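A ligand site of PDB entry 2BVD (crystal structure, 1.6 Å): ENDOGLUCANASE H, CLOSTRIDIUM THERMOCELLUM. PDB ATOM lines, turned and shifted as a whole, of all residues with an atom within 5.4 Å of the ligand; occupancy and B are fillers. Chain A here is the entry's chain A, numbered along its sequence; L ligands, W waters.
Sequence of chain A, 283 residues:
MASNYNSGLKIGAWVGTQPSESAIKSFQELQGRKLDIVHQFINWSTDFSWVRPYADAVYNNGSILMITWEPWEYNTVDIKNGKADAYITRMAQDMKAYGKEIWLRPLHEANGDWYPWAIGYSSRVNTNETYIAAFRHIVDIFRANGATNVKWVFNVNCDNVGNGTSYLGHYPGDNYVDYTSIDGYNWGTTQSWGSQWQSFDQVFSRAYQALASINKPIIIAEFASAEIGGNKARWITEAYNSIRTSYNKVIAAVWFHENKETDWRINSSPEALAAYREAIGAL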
ATOM      1  N   TRP A  14      10.897   4.521 -34.129  1.00  0.00           N
ATOM      2  CA  TRP A  14      11.974   3.602 -34.521  1.00  0.00           C
ATOM      3  C   TRP A  14      11.607   2.254 -33.906  1.00  0.00           C
ATOM      4  O   TRP A  14      11.542   2.146 -32.677  1.00  0.00           O
ATOM      5  CB  TRP A  14      13.329   4.077 -33.981  1.00  0.00           C
ATOM      6  CG  TRP A  14      14.328   2.984 -33.697  1.00  0.00           C
ATOM      7  CD1 TRP A  14      14.691   2.489 -32.473  1.00  0.00           C
ATOM      8  CD2 TRP A  14      15.125   2.282 -34.664  1.00  0.00           C
ATOM      9  NE1 TRP A  14      15.646   1.518 -32.612  1.00  0.00           N
ATOM     10  CE2 TRP A  14      15.945   1.366 -33.949  1.00  0.00           C
ATOM     11  CE3 TRP A  14      15.244   2.334 -36.056  1.00  0.00           C
ATOM     12  CZ2 TRP A  14      16.844   0.500 -34.585  1.00  0.00           C
ATOM     13  CZ3 TRP A  14      16.140   1.477 -36.695  1.00  0.00           C
ATOM     14  CH2 TRP A  14      16.928   0.569 -35.949  1.00  0.00           C
ATOM     15  N   PHE A  41      17.800   4.791 -38.550  1.00  0.00           N
ATOM     16  CA  PHE A  41      19.139   5.376 -38.432  1.00  0.00           C
ATOM     17  C   PHE A  41      20.050   4.779 -39.487  1.00  0.00           C
ATOM     18  O   PHE A  41      20.048   3.572 -39.704  1.00  0.00           O
ATOM     19  CB  PHE A  41      19.751   5.083 -37.056  1.00  0.00           C
ATOM     20  CG  PHE A  41      18.977   5.678 -35.899  1.00  0.00           C
ATOM     21  CD1 PHE A  41      17.827   5.050 -35.421  1.00  0.00           C
ATOM     22  CD2 PHE A  41      19.400   6.851 -35.290  1.00  0.00           C
ATOM     23  CE1 PHE A  41      17.099   5.584 -34.365  1.00  0.00           C
ATOM     24  CE2 PHE A  41      18.687   7.395 -34.221  1.00  0.00           C
ATOM     25  CZ  PHE A  41      17.540   6.765 -33.753  1.00  0.00           C
ATOM     26  N   GLU A  70      23.719   9.696 -39.585  1.00  0.00           N
ATOM     27  CA  GLU A  70      24.772   9.803 -38.558  1.00  0.00           C
ATOM     28  C   GLU A  70      26.171   9.769 -39.155  1.00  0.00           C
ATOM     29  O   GLU A  70      26.630   8.699 -39.560  1.00  0.00           O
ATOM     30  CB  GLU A  70      24.652   8.642 -37.564  1.00  0.00           C
ATOM     31  CG  GLU A  70      23.310   8.554 -36.859  1.00  0.00           C
ATOM     32  CD  GLU A  70      23.342   7.525 -35.745  1.00  0.00           C
ATOM     33  OE1 GLU A  70      23.923   6.430 -35.961  1.00  0.00           O
ATOM     34  OE2 GLU A  70      22.783   7.794 -34.667  1.00  0.00           O
ATOM     35  N   TRP A  72      29.289   9.132 -38.526  1.00  0.00           N
ATOM     36  CA  TRP A  72      30.400   8.542 -37.771  1.00  0.00           C
ATOM     37  C   TRP A  72      31.697   8.694 -38.567  1.00  0.00           C
ATOM     38  O   TRP A  72      32.785   8.831 -37.994  1.00  0.00           O
ATOM     39  CB  TRP A  72      30.139   7.066 -37.490  1.00  0.00           C
ATOM     40  CG  TRP A  72      28.919   6.847 -36.647  1.00  0.00           C
ATOM     41  CD1 TRP A  72      27.679   6.526 -37.093  1.00  0.00           C
ATOM     42  CD2 TRP A  72      28.827   6.942 -35.216  1.00  0.00           C
ATOM     43  NE1 TRP A  72      26.810   6.401 -36.034  1.00  0.00           N
ATOM     44  CE2 TRP A  72      27.480   6.664 -34.873  1.00  0.00           C
ATOM     45  CE3 TRP A  72      29.729   7.245 -34.201  1.00  0.00           C
ATOM     46  CZ2 TRP A  72      27.031   6.656 -33.542  1.00  0.00           C
ATOM     47  CZ3 TRP A  72      29.280   7.237 -32.869  1.00  0.00           C
ATOM     48  CH2 TRP A  72      27.940   6.960 -32.567  1.00  0.00           C
ATOM     49  N   HIS A 108      22.754  14.831 -35.394  1.00  0.00           N
ATOM     50  CA  HIS A 108      21.779  15.207 -34.361  1.00  0.00           C
ATOM     51  C   HIS A 108      22.390  15.281 -32.961  1.00  0.00           C
ATOM     52  O   HIS A 108      23.608  15.195 -32.800  1.00  0.00           O
ATOM     53  CB  HIS A 108      20.582  14.261 -34.378  1.00  0.00           C
ATOM     54  CG  HIS A 108      20.890  12.887 -33.874  1.00  0.00           C
ATOM     55  ND1 HIS A 108      21.835  12.068 -34.454  1.00  0.00           N
ATOM     56  CD2 HIS A 108      20.357  12.171 -32.852  1.00  0.00           C
ATOM     57  CE1 HIS A 108      21.892  10.926 -33.807  1.00  0.00           C
ATOM     58  NE2 HIS A 108      21.000  10.958 -32.822  1.00  0.00           N
ATOM     59  N   GLU A 109      21.540  15.466 -31.967  1.00  0.00           N
ATOM     60  CA  GLU A 109      21.977  15.531 -30.561  1.00  0.00           C
ATOM     61  C   GLU A 109      23.340  16.200 -30.424  1.00  0.00           C
ATOM     62  O   GLU A 109      24.175  15.784 -29.605  1.00  0.00           O
ATOM     63  CB  GLU A 109      21.946  14.139 -29.925  1.00  0.00           C
ATOM     64  CG  GLU A 109      20.505  13.637 -29.676  1.00  0.00           C
ATOM     65  CD  GLU A 109      20.416  12.163 -29.251  1.00  0.00           C
ATOM     66  OE1 GLU A 109      21.448  11.515 -29.015  1.00  0.00           O
ATOM     67  OE2 GLU A 109      19.276  11.663 -29.140  1.00  0.00           O
ATOM     68  N   TRP A 114      28.287  12.743 -26.866  1.00  0.00           N
ATOM     69  CA  TRP A 114      28.508  11.334 -27.208  1.00  0.00           C
ATOM     70  C   TRP A 114      28.775  11.058 -28.676  1.00  0.00           C
ATOM     71  O   TRP A 114      29.277   9.992 -29.017  1.00  0.00           O
ATOM     72  CB  TRP A 114      27.377  10.447 -26.688  1.00  0.00           C
ATOM     73  CG  TRP A 114      25.991  10.975 -26.943  1.00  0.00           C
ATOM     74  CD1 TRP A 114      25.222  10.760 -28.047  1.00  0.00           C
ATOM     75  CD2 TRP A 114      25.224  11.788 -26.046  1.00  0.00           C
ATOM     76  NE1 TRP A 114      24.003  11.398 -27.897  1.00  0.00           N
ATOM     77  CE2 TRP A 114      23.976  12.038 -26.688  1.00  0.00           C
ATOM     78  CE3 TRP A 114      25.459  12.337 -24.774  1.00  0.00           C
ATOM     79  CZ2 TRP A 114      22.961  12.805 -26.084  1.00  0.00           C
ATOM     80  CZ3 TRP A 114      24.459  13.096 -24.175  1.00  0.00           C
ATOM     81  CH2 TRP A 114      23.232  13.335 -24.841  1.00  0.00           C
ATOM     82  N   TYR A 115      28.427  12.001 -29.551  1.00  0.00           N
ATOM     83  CA  TYR A 115      28.677  11.786 -30.952  1.00  0.00           C
ATOM     84  C   TYR A 115      29.906  12.565 -31.441  1.00  0.00           C
ATOM     85  O   TYR A 115      30.162  13.665 -30.958  1.00  0.00           O
ATOM     86  CB  TYR A 115      27.462  12.230 -31.756  1.00  0.00           C
ATOM     87  CG  TYR A 115      26.238  11.352 -31.605  1.00  0.00           C
ATOM     88  CD1 TYR A 115      26.333   9.966 -31.733  1.00  0.00           C
ATOM     89  CD2 TYR A 115      24.984  11.917 -31.395  1.00  0.00           C
ATOM     90  CE1 TYR A 115      25.217   9.161 -31.621  1.00  0.00           C
ATOM     91  CE2 TYR A 115      23.850  11.104 -31.286  1.00  0.00           C
ATOM     92  CZ  TYR A 115      23.981   9.734 -31.408  1.00  0.00           C
ATOM     93  OH  TYR A 115      22.858   8.947 -31.301  1.00  0.00           O
ATOM     94  N   ASP A 183      15.006  15.199 -28.431  1.00  0.00           N
ATOM     95  CA  ASP A 183      15.115  13.814 -27.970  1.00  0.00           C
ATOM     96  C   ASP A 183      15.203  13.817 -26.447  1.00  0.00           C
ATOM     97  O   ASP A 183      15.839  14.694 -25.860  1.00  0.00           O
ATOM     98  CB  ASP A 183      16.387  13.144 -28.513  1.00  0.00           C
ATOM     99  CG  ASP A 183      16.380  12.999 -30.013  1.00  0.00           C
ATOM    100  OD1 ASP A 183      15.396  13.370 -30.694  1.00  0.00           O
ATOM    101  OD2 ASP A 183      17.391  12.489 -30.549  1.00  0.00           O
ATOM    102  N   TYR A 185      14.685  11.014 -22.727  1.00  0.00           N
ATOM    103  CA  TYR A 185      14.366   9.719 -22.142  1.00  0.00           C
ATOM    104  C   TYR A 185      14.180   9.847 -20.639  1.00  0.00           C
ATOM    105  O   TYR A 185      14.936  10.565 -19.960  1.00  0.00           O
ATOM    106  CB  TYR A 185      15.516   8.748 -22.438  1.00  0.00           C
ATOM    107  CG  TYR A 185      15.617   8.367 -23.897  1.00  0.00           C
ATOM    108  CD1 TYR A 185      15.118   7.150 -24.347  1.00  0.00           C
ATOM    109  CD2 TYR A 185      16.201   9.232 -24.831  1.00  0.00           C
ATOM    110  CE1 TYR A 185      15.191   6.786 -25.690  1.00  0.00           C
ATOM    111  CE2 TYR A 185      16.273   8.881 -26.199  1.00  0.00           C
ATOM    112  CZ  TYR A 185      15.758   7.660 -26.611  1.00  0.00           C
ATOM    113  OH  TYR A 185      15.817   7.289 -27.924  1.00  0.00           O
ATOM    114  N   TRP A 187      15.039   7.867 -17.780  1.00  0.00           N
ATOM    115  CA  TRP A 187      15.916   6.753 -17.451  1.00  0.00           C
ATOM    116  C   TRP A 187      15.482   5.995 -16.200  1.00  0.00           C
ATOM    117  O   TRP A 187      16.022   4.933 -15.904  1.00  0.00           O
ATOM    118  CB  TRP A 187      17.341   7.286 -17.255  1.00  0.00           C
ATOM    119  CG  TRP A 187      17.919   7.849 -18.516  1.00  0.00           C
ATOM    120  CD1 TRP A 187      17.783   9.122 -18.981  1.00  0.00           C
ATOM    121  CD2 TRP A 187      18.705   7.145 -19.475  1.00  0.00           C
ATOM    122  NE1 TRP A 187      18.454   9.272 -20.176  1.00  0.00           N
ATOM    123  CE2 TRP A 187      19.027   8.068 -20.508  1.00  0.00           C
ATOM    124  CE3 TRP A 187      19.177   5.823 -19.575  1.00  0.00           C
ATOM    125  CZ2 TRP A 187      19.802   7.701 -21.621  1.00  0.00           C
ATOM    126  CZ3 TRP A 187      19.946   5.467 -20.682  1.00  0.00           C
ATOM    127  CH2 TRP A 187      20.256   6.405 -21.689  1.00  0.00           C
ATOM    128  N   GLU A 222      12.847  11.335 -30.675  1.00  0.00           N
ATOM    129  CA  GLU A 222      13.126  10.134 -29.889  1.00  0.00           C
ATOM    130  C   GLU A 222      12.622  10.374 -28.491  1.00  0.00           C
ATOM    131  O   GLU A 222      13.009  11.364 -27.851  1.00  0.00           O
ATOM    132  CB  GLU A 222      14.620   9.839 -29.763  1.00  0.00           C
ATOM    133  CG  GLU A 222      15.378   9.586 -31.055  1.00  0.00           C
ATOM    134  CD  GLU A 222      16.835   9.238 -30.779  1.00  0.00           C
ATOM    135  OE1 GLU A 222      17.141   8.747 -29.678  1.00  0.00           O
ATOM    136  OE2 GLU A 222      17.681   9.491 -31.661  1.00  0.00           O
ATOM    137  N   PHE A 256      11.028   5.588 -29.272  1.00  0.00           N
ATOM    138  CA  PHE A 256      12.232   4.799 -29.520  1.00  0.00           C
ATOM    139  C   PHE A 256      11.998   3.407 -28.920  1.00  0.00           C
ATOM    140  O   PHE A 256      12.164   3.219 -27.725  1.00  0.00           O
ATOM    141  CB  PHE A 256      13.440   5.488 -28.878  1.00  0.00           C
ATOM    142  CG  PHE A 256      14.764   4.851 -29.180  1.00  0.00           C
ATOM    143  CD1 PHE A 256      15.487   5.210 -30.312  1.00  0.00           C
ATOM    144  CD2 PHE A 256      15.351   3.962 -28.282  1.00  0.00           C
ATOM    145  CE1 PHE A 256      16.744   4.660 -30.577  1.00  0.00           C
ATOM    146  CE2 PHE A 256      16.590   3.398 -28.538  1.00  0.00           C
ATOM    147  CZ  PHE A 256      17.294   3.755 -29.686  1.00  0.00           C
ATOM    148  N   GLU A 258      13.160   0.011 -28.431  1.00  0.00           N
ATOM    149  CA  GLU A 258      14.260  -0.963 -28.443  1.00  0.00           C
ATOM    150  C   GLU A 258      14.626  -1.328 -27.003  1.00  0.00           C
ATOM    151  O   GLU A 258      14.617  -0.467 -26.126  1.00  0.00           O
ATOM    152  CB  GLU A 258      15.474  -0.374 -29.181  1.00  0.00           C
ATOM    153  CG  GLU A 258      16.517  -1.416 -29.566  1.00  0.00           C
ATOM    154  CD  GLU A 258      17.735  -0.825 -30.270  1.00  0.00           C
ATOM    155  OE1 GLU A 258      17.587   0.231 -30.933  1.00  0.00           O
ATOM    156  OE2 GLU A 258      18.836  -1.423 -30.165  1.00  0.00           O
ATOM    157  N   LYS A 260      17.449  -1.720 -25.098  1.00  0.00           N
ATOM    158  CA  LYS A 260      18.818  -1.275 -25.302  1.00  0.00           C
ATOM    159  C   LYS A 260      19.464  -0.904 -23.960  1.00  0.00           C
ATOM    160  O   LYS A 260      19.750  -1.805 -23.154  1.00  0.00           O
ATOM    161  CB  LYS A 260      18.832  -0.116 -26.315  1.00  0.00           C
ATOM    162  CG  LYS A 260      20.190   0.134 -26.956  1.00  0.00           C
ATOM    163  CD  LYS A 260      20.093   1.288 -27.957  1.00  0.00           C
ATOM    164  CE  LYS A 260      21.443   1.544 -28.570  1.00  0.00           C
ATOM    165  NZ  LYS A 260      21.399   2.635 -29.584  1.00  0.00           N
ATOM    166  N   GLU A 261      19.665   0.383 -23.694  1.00  0.00           N
ATOM    167  CA  GLU A 261      20.299   0.812 -22.432  1.00  0.00           C
ATOM    168  C   GLU A 261      19.430   0.390 -21.253  1.00  0.00           C
ATOM    169  O   GLU A 261      19.933   0.060 -20.165  1.00  0.00           O
ATOM    170  CB  GLU A 261      20.534   2.323 -22.410  1.00  0.00           C
ATOM    171  CG  GLU A 261      21.475   2.823 -23.502  1.00  0.00           C
ATOM    172  CD  GLU A 261      20.767   3.245 -24.785  1.00  0.00           C
ATOM    173  OE1 GLU A 261      19.595   2.849 -24.995  1.00  0.00           O
ATOM    174  OE2 GLU A 261      21.404   3.985 -25.582  1.00  0.00           O
ATOM    175  N   TRP A 264      13.187   0.240 -23.276  1.00  0.00           N
ATOM    176  CA  TRP A 264      12.414   1.378 -23.751  1.00  0.00           C
ATOM    177  C   TRP A 264      11.113   0.936 -24.422  1.00  0.00           C
ATOM    178  O   TRP A 264      10.224   1.762 -24.657  1.00  0.00           O
ATOM    179  CB  TRP A 264      13.220   2.160 -24.785  1.00  0.00           C
ATOM    180  CG  TRP A 264      14.569   2.665 -24.349  1.00  0.00           C
ATOM    181  CD1 TRP A 264      15.776   2.383 -24.934  1.00  0.00           C
ATOM    182  CD2 TRP A 264      14.856   3.569 -23.250  1.00  0.00           C
ATOM    183  NE1 TRP A 264      16.792   3.055 -24.289  1.00  0.00           N
ATOM    184  CE2 TRP A 264      16.259   3.780 -23.253  1.00  0.00           C
ATOM    185  CE3 TRP A 264      14.068   4.227 -22.292  1.00  0.00           C
ATOM    186  CZ2 TRP A 264      16.894   4.616 -22.317  1.00  0.00           C
ATOM    187  CZ3 TRP A 264      14.703   5.056 -21.343  1.00  0.00           C
ATOM    188  CH2 TRP A 264      16.101   5.244 -21.375  1.00  0.00           C
HETATM  189  O1  LIG L   1      20.597   6.797 -25.137  1.00  0.00           O
HETATM  190  C1  LIG L   1      20.461   8.025 -29.770  1.00  0.00           C
HETATM  191  N1  LIG L   1      19.639   8.796 -28.836  1.00  0.00           N
HETATM  192  C2  LIG L   1      20.349   6.509 -29.544  1.00  0.00           C
HETATM  193  O2  LIG L   1      21.451   5.876 -30.217  1.00  0.00           O
HETATM  194  C3  LIG L   1      20.455   6.120 -28.076  1.00  0.00           C
HETATM  195  O3  LIG L   1      20.238   4.709 -27.956  1.00  0.00           O
HETATM  196  C4  LIG L   1      19.435   6.940 -27.272  1.00  0.00           C
HETATM  197  C5  LIG L   1      19.711   8.431 -27.425  1.00  0.00           C
HETATM  198  C6  LIG L   1      21.131   5.520 -31.556  1.00  0.00           C
HETATM  199  C7  LIG L   1      22.443   5.322 -32.311  1.00  0.00           C
HETATM  200  O4  LIG L   1      23.153   6.572 -32.436  1.00  0.00           O
HETATM  201  C8  LIG L   1      22.221   4.680 -33.674  1.00  0.00           C
HETATM  202  O5  LIG L   1      23.492   4.378 -34.258  1.00  0.00           O
HETATM  203  C9  LIG L   1      21.363   3.415 -33.556  1.00  0.00           C
HETATM  204  O6  LIG L   1      21.087   2.866 -34.849  1.00  0.00           O
HETATM  205  C10 LIG L   1      20.066   3.791 -32.826  1.00  0.00           C
HETATM  206  C11 LIG L   1      19.345   6.561 -25.787  1.00  0.00           C
HETATM  207  C12 LIG L   1      19.137   2.604 -32.628  1.00  0.00           C
HETATM  208  O7  LIG L   1      19.747   1.700 -31.699  1.00  0.00           O
HETATM  209  O8  LIG L   1      20.413   4.284 -31.543  1.00  0.00           O
HETATM  210  O   HOH W   1      20.986   0.135 -34.515  1.00  0.00           O
HETATM  211  O   HOH W   2      20.193  -1.653 -32.378  1.00  0.00           O
HETATM  212  O   HOH W   3      25.086   2.783 -33.033  1.00  0.00           O
HETATM  213  O   HOH W   4      22.552   2.800 -37.196  1.00  0.00           O
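The side-chain carboxylate (OE2) of Glu 70 is in hydrogen-bond range of an oxygen (O4) of the ligand (2.6 Å).
OE1 of Glu 222 is in salt-bridge range of N1 of the ligand (2.6 Å).
O4 of the ligand sits at hydrogen-bond distance from OH of Tyr 115 (2.6 Å).
The side-chain carboxylate (OE1) of Glu 258 sits at hydrogen-bond distance from an oxygen (O7) of the ligand (2.7 Å).
The side-chain carboxylate of Glu 261 lies within hydrogen-bond range of an oxygen (O3) of the ligand (2.7 Å).
An oxygen (O8) of the ligand sits at hydrogen-bond distance from the side-chain amino group (NZ) of Lys 260 (2.7 Å).
N1 of the ligand lies within salt-bridge range of OE2 of Glu 109 (2.9 Å).
The side-chain carboxylate (OE1) of Glu 70 lies within hydrogen-bond range of the indole nitrogen (NE1) of Trp 72, 2.9 Å away.
OE1 of Glu 222 sits at hydrogen-bond distance from OH of Tyr 185, at 2.6 Å.
The backbone NH (N) of Glu 222 is in hydrogen-bond range of the side-chain carboxylate (OD1) of Asp 183.
OH of Tyr 115 sits at hydrogen-bond distance from NE2 of His 108 (3.1 Å).
The indole nitrogen (NE1) of Trp 14 sits at hydrogen-bond distance from the side-chain carboxylate (OE1) of Glu 258, 2.9 Å away.
NE1 of Trp 264 is in hydrogen-bond range of OE1 of Glu 261 (2.9 Å).
OE2 of Glu 109 lies close to OD2 of Asp 183, at 2.5 Å.
The side-chain carboxylate of Glu 109 is in hydrogen-bond range of the indole nitrogen of Trp 114.
Trp 14 touches the ligand (NE1 to C12, 3.7 Å).
CB of Phe 41 touches O6 of the ligand, 3.4 Å away.
CE2 of Tyr 185 touches C5 of the ligand (3.7 Å).
Trp 187 touches the ligand.
CZ of Phe 256 touches O3 of the ligand, 3.5 Å away.
Hydrophobic or aromatic side chains within 4 Å of the ligand: Trp 14, Phe 41, Tyr 115, Tyr 185, Trp 187 and Phe 256.
Of the 17 residues printed, 12 come within 4 Å of the ligand.
The nearest printed residue that does not touch the ligand is Trp 72 (4.03 Å).
Water W2 bridges the side-chain carboxylate (OE2) of Glu 258 and an oxygen (O7) of the ligand.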
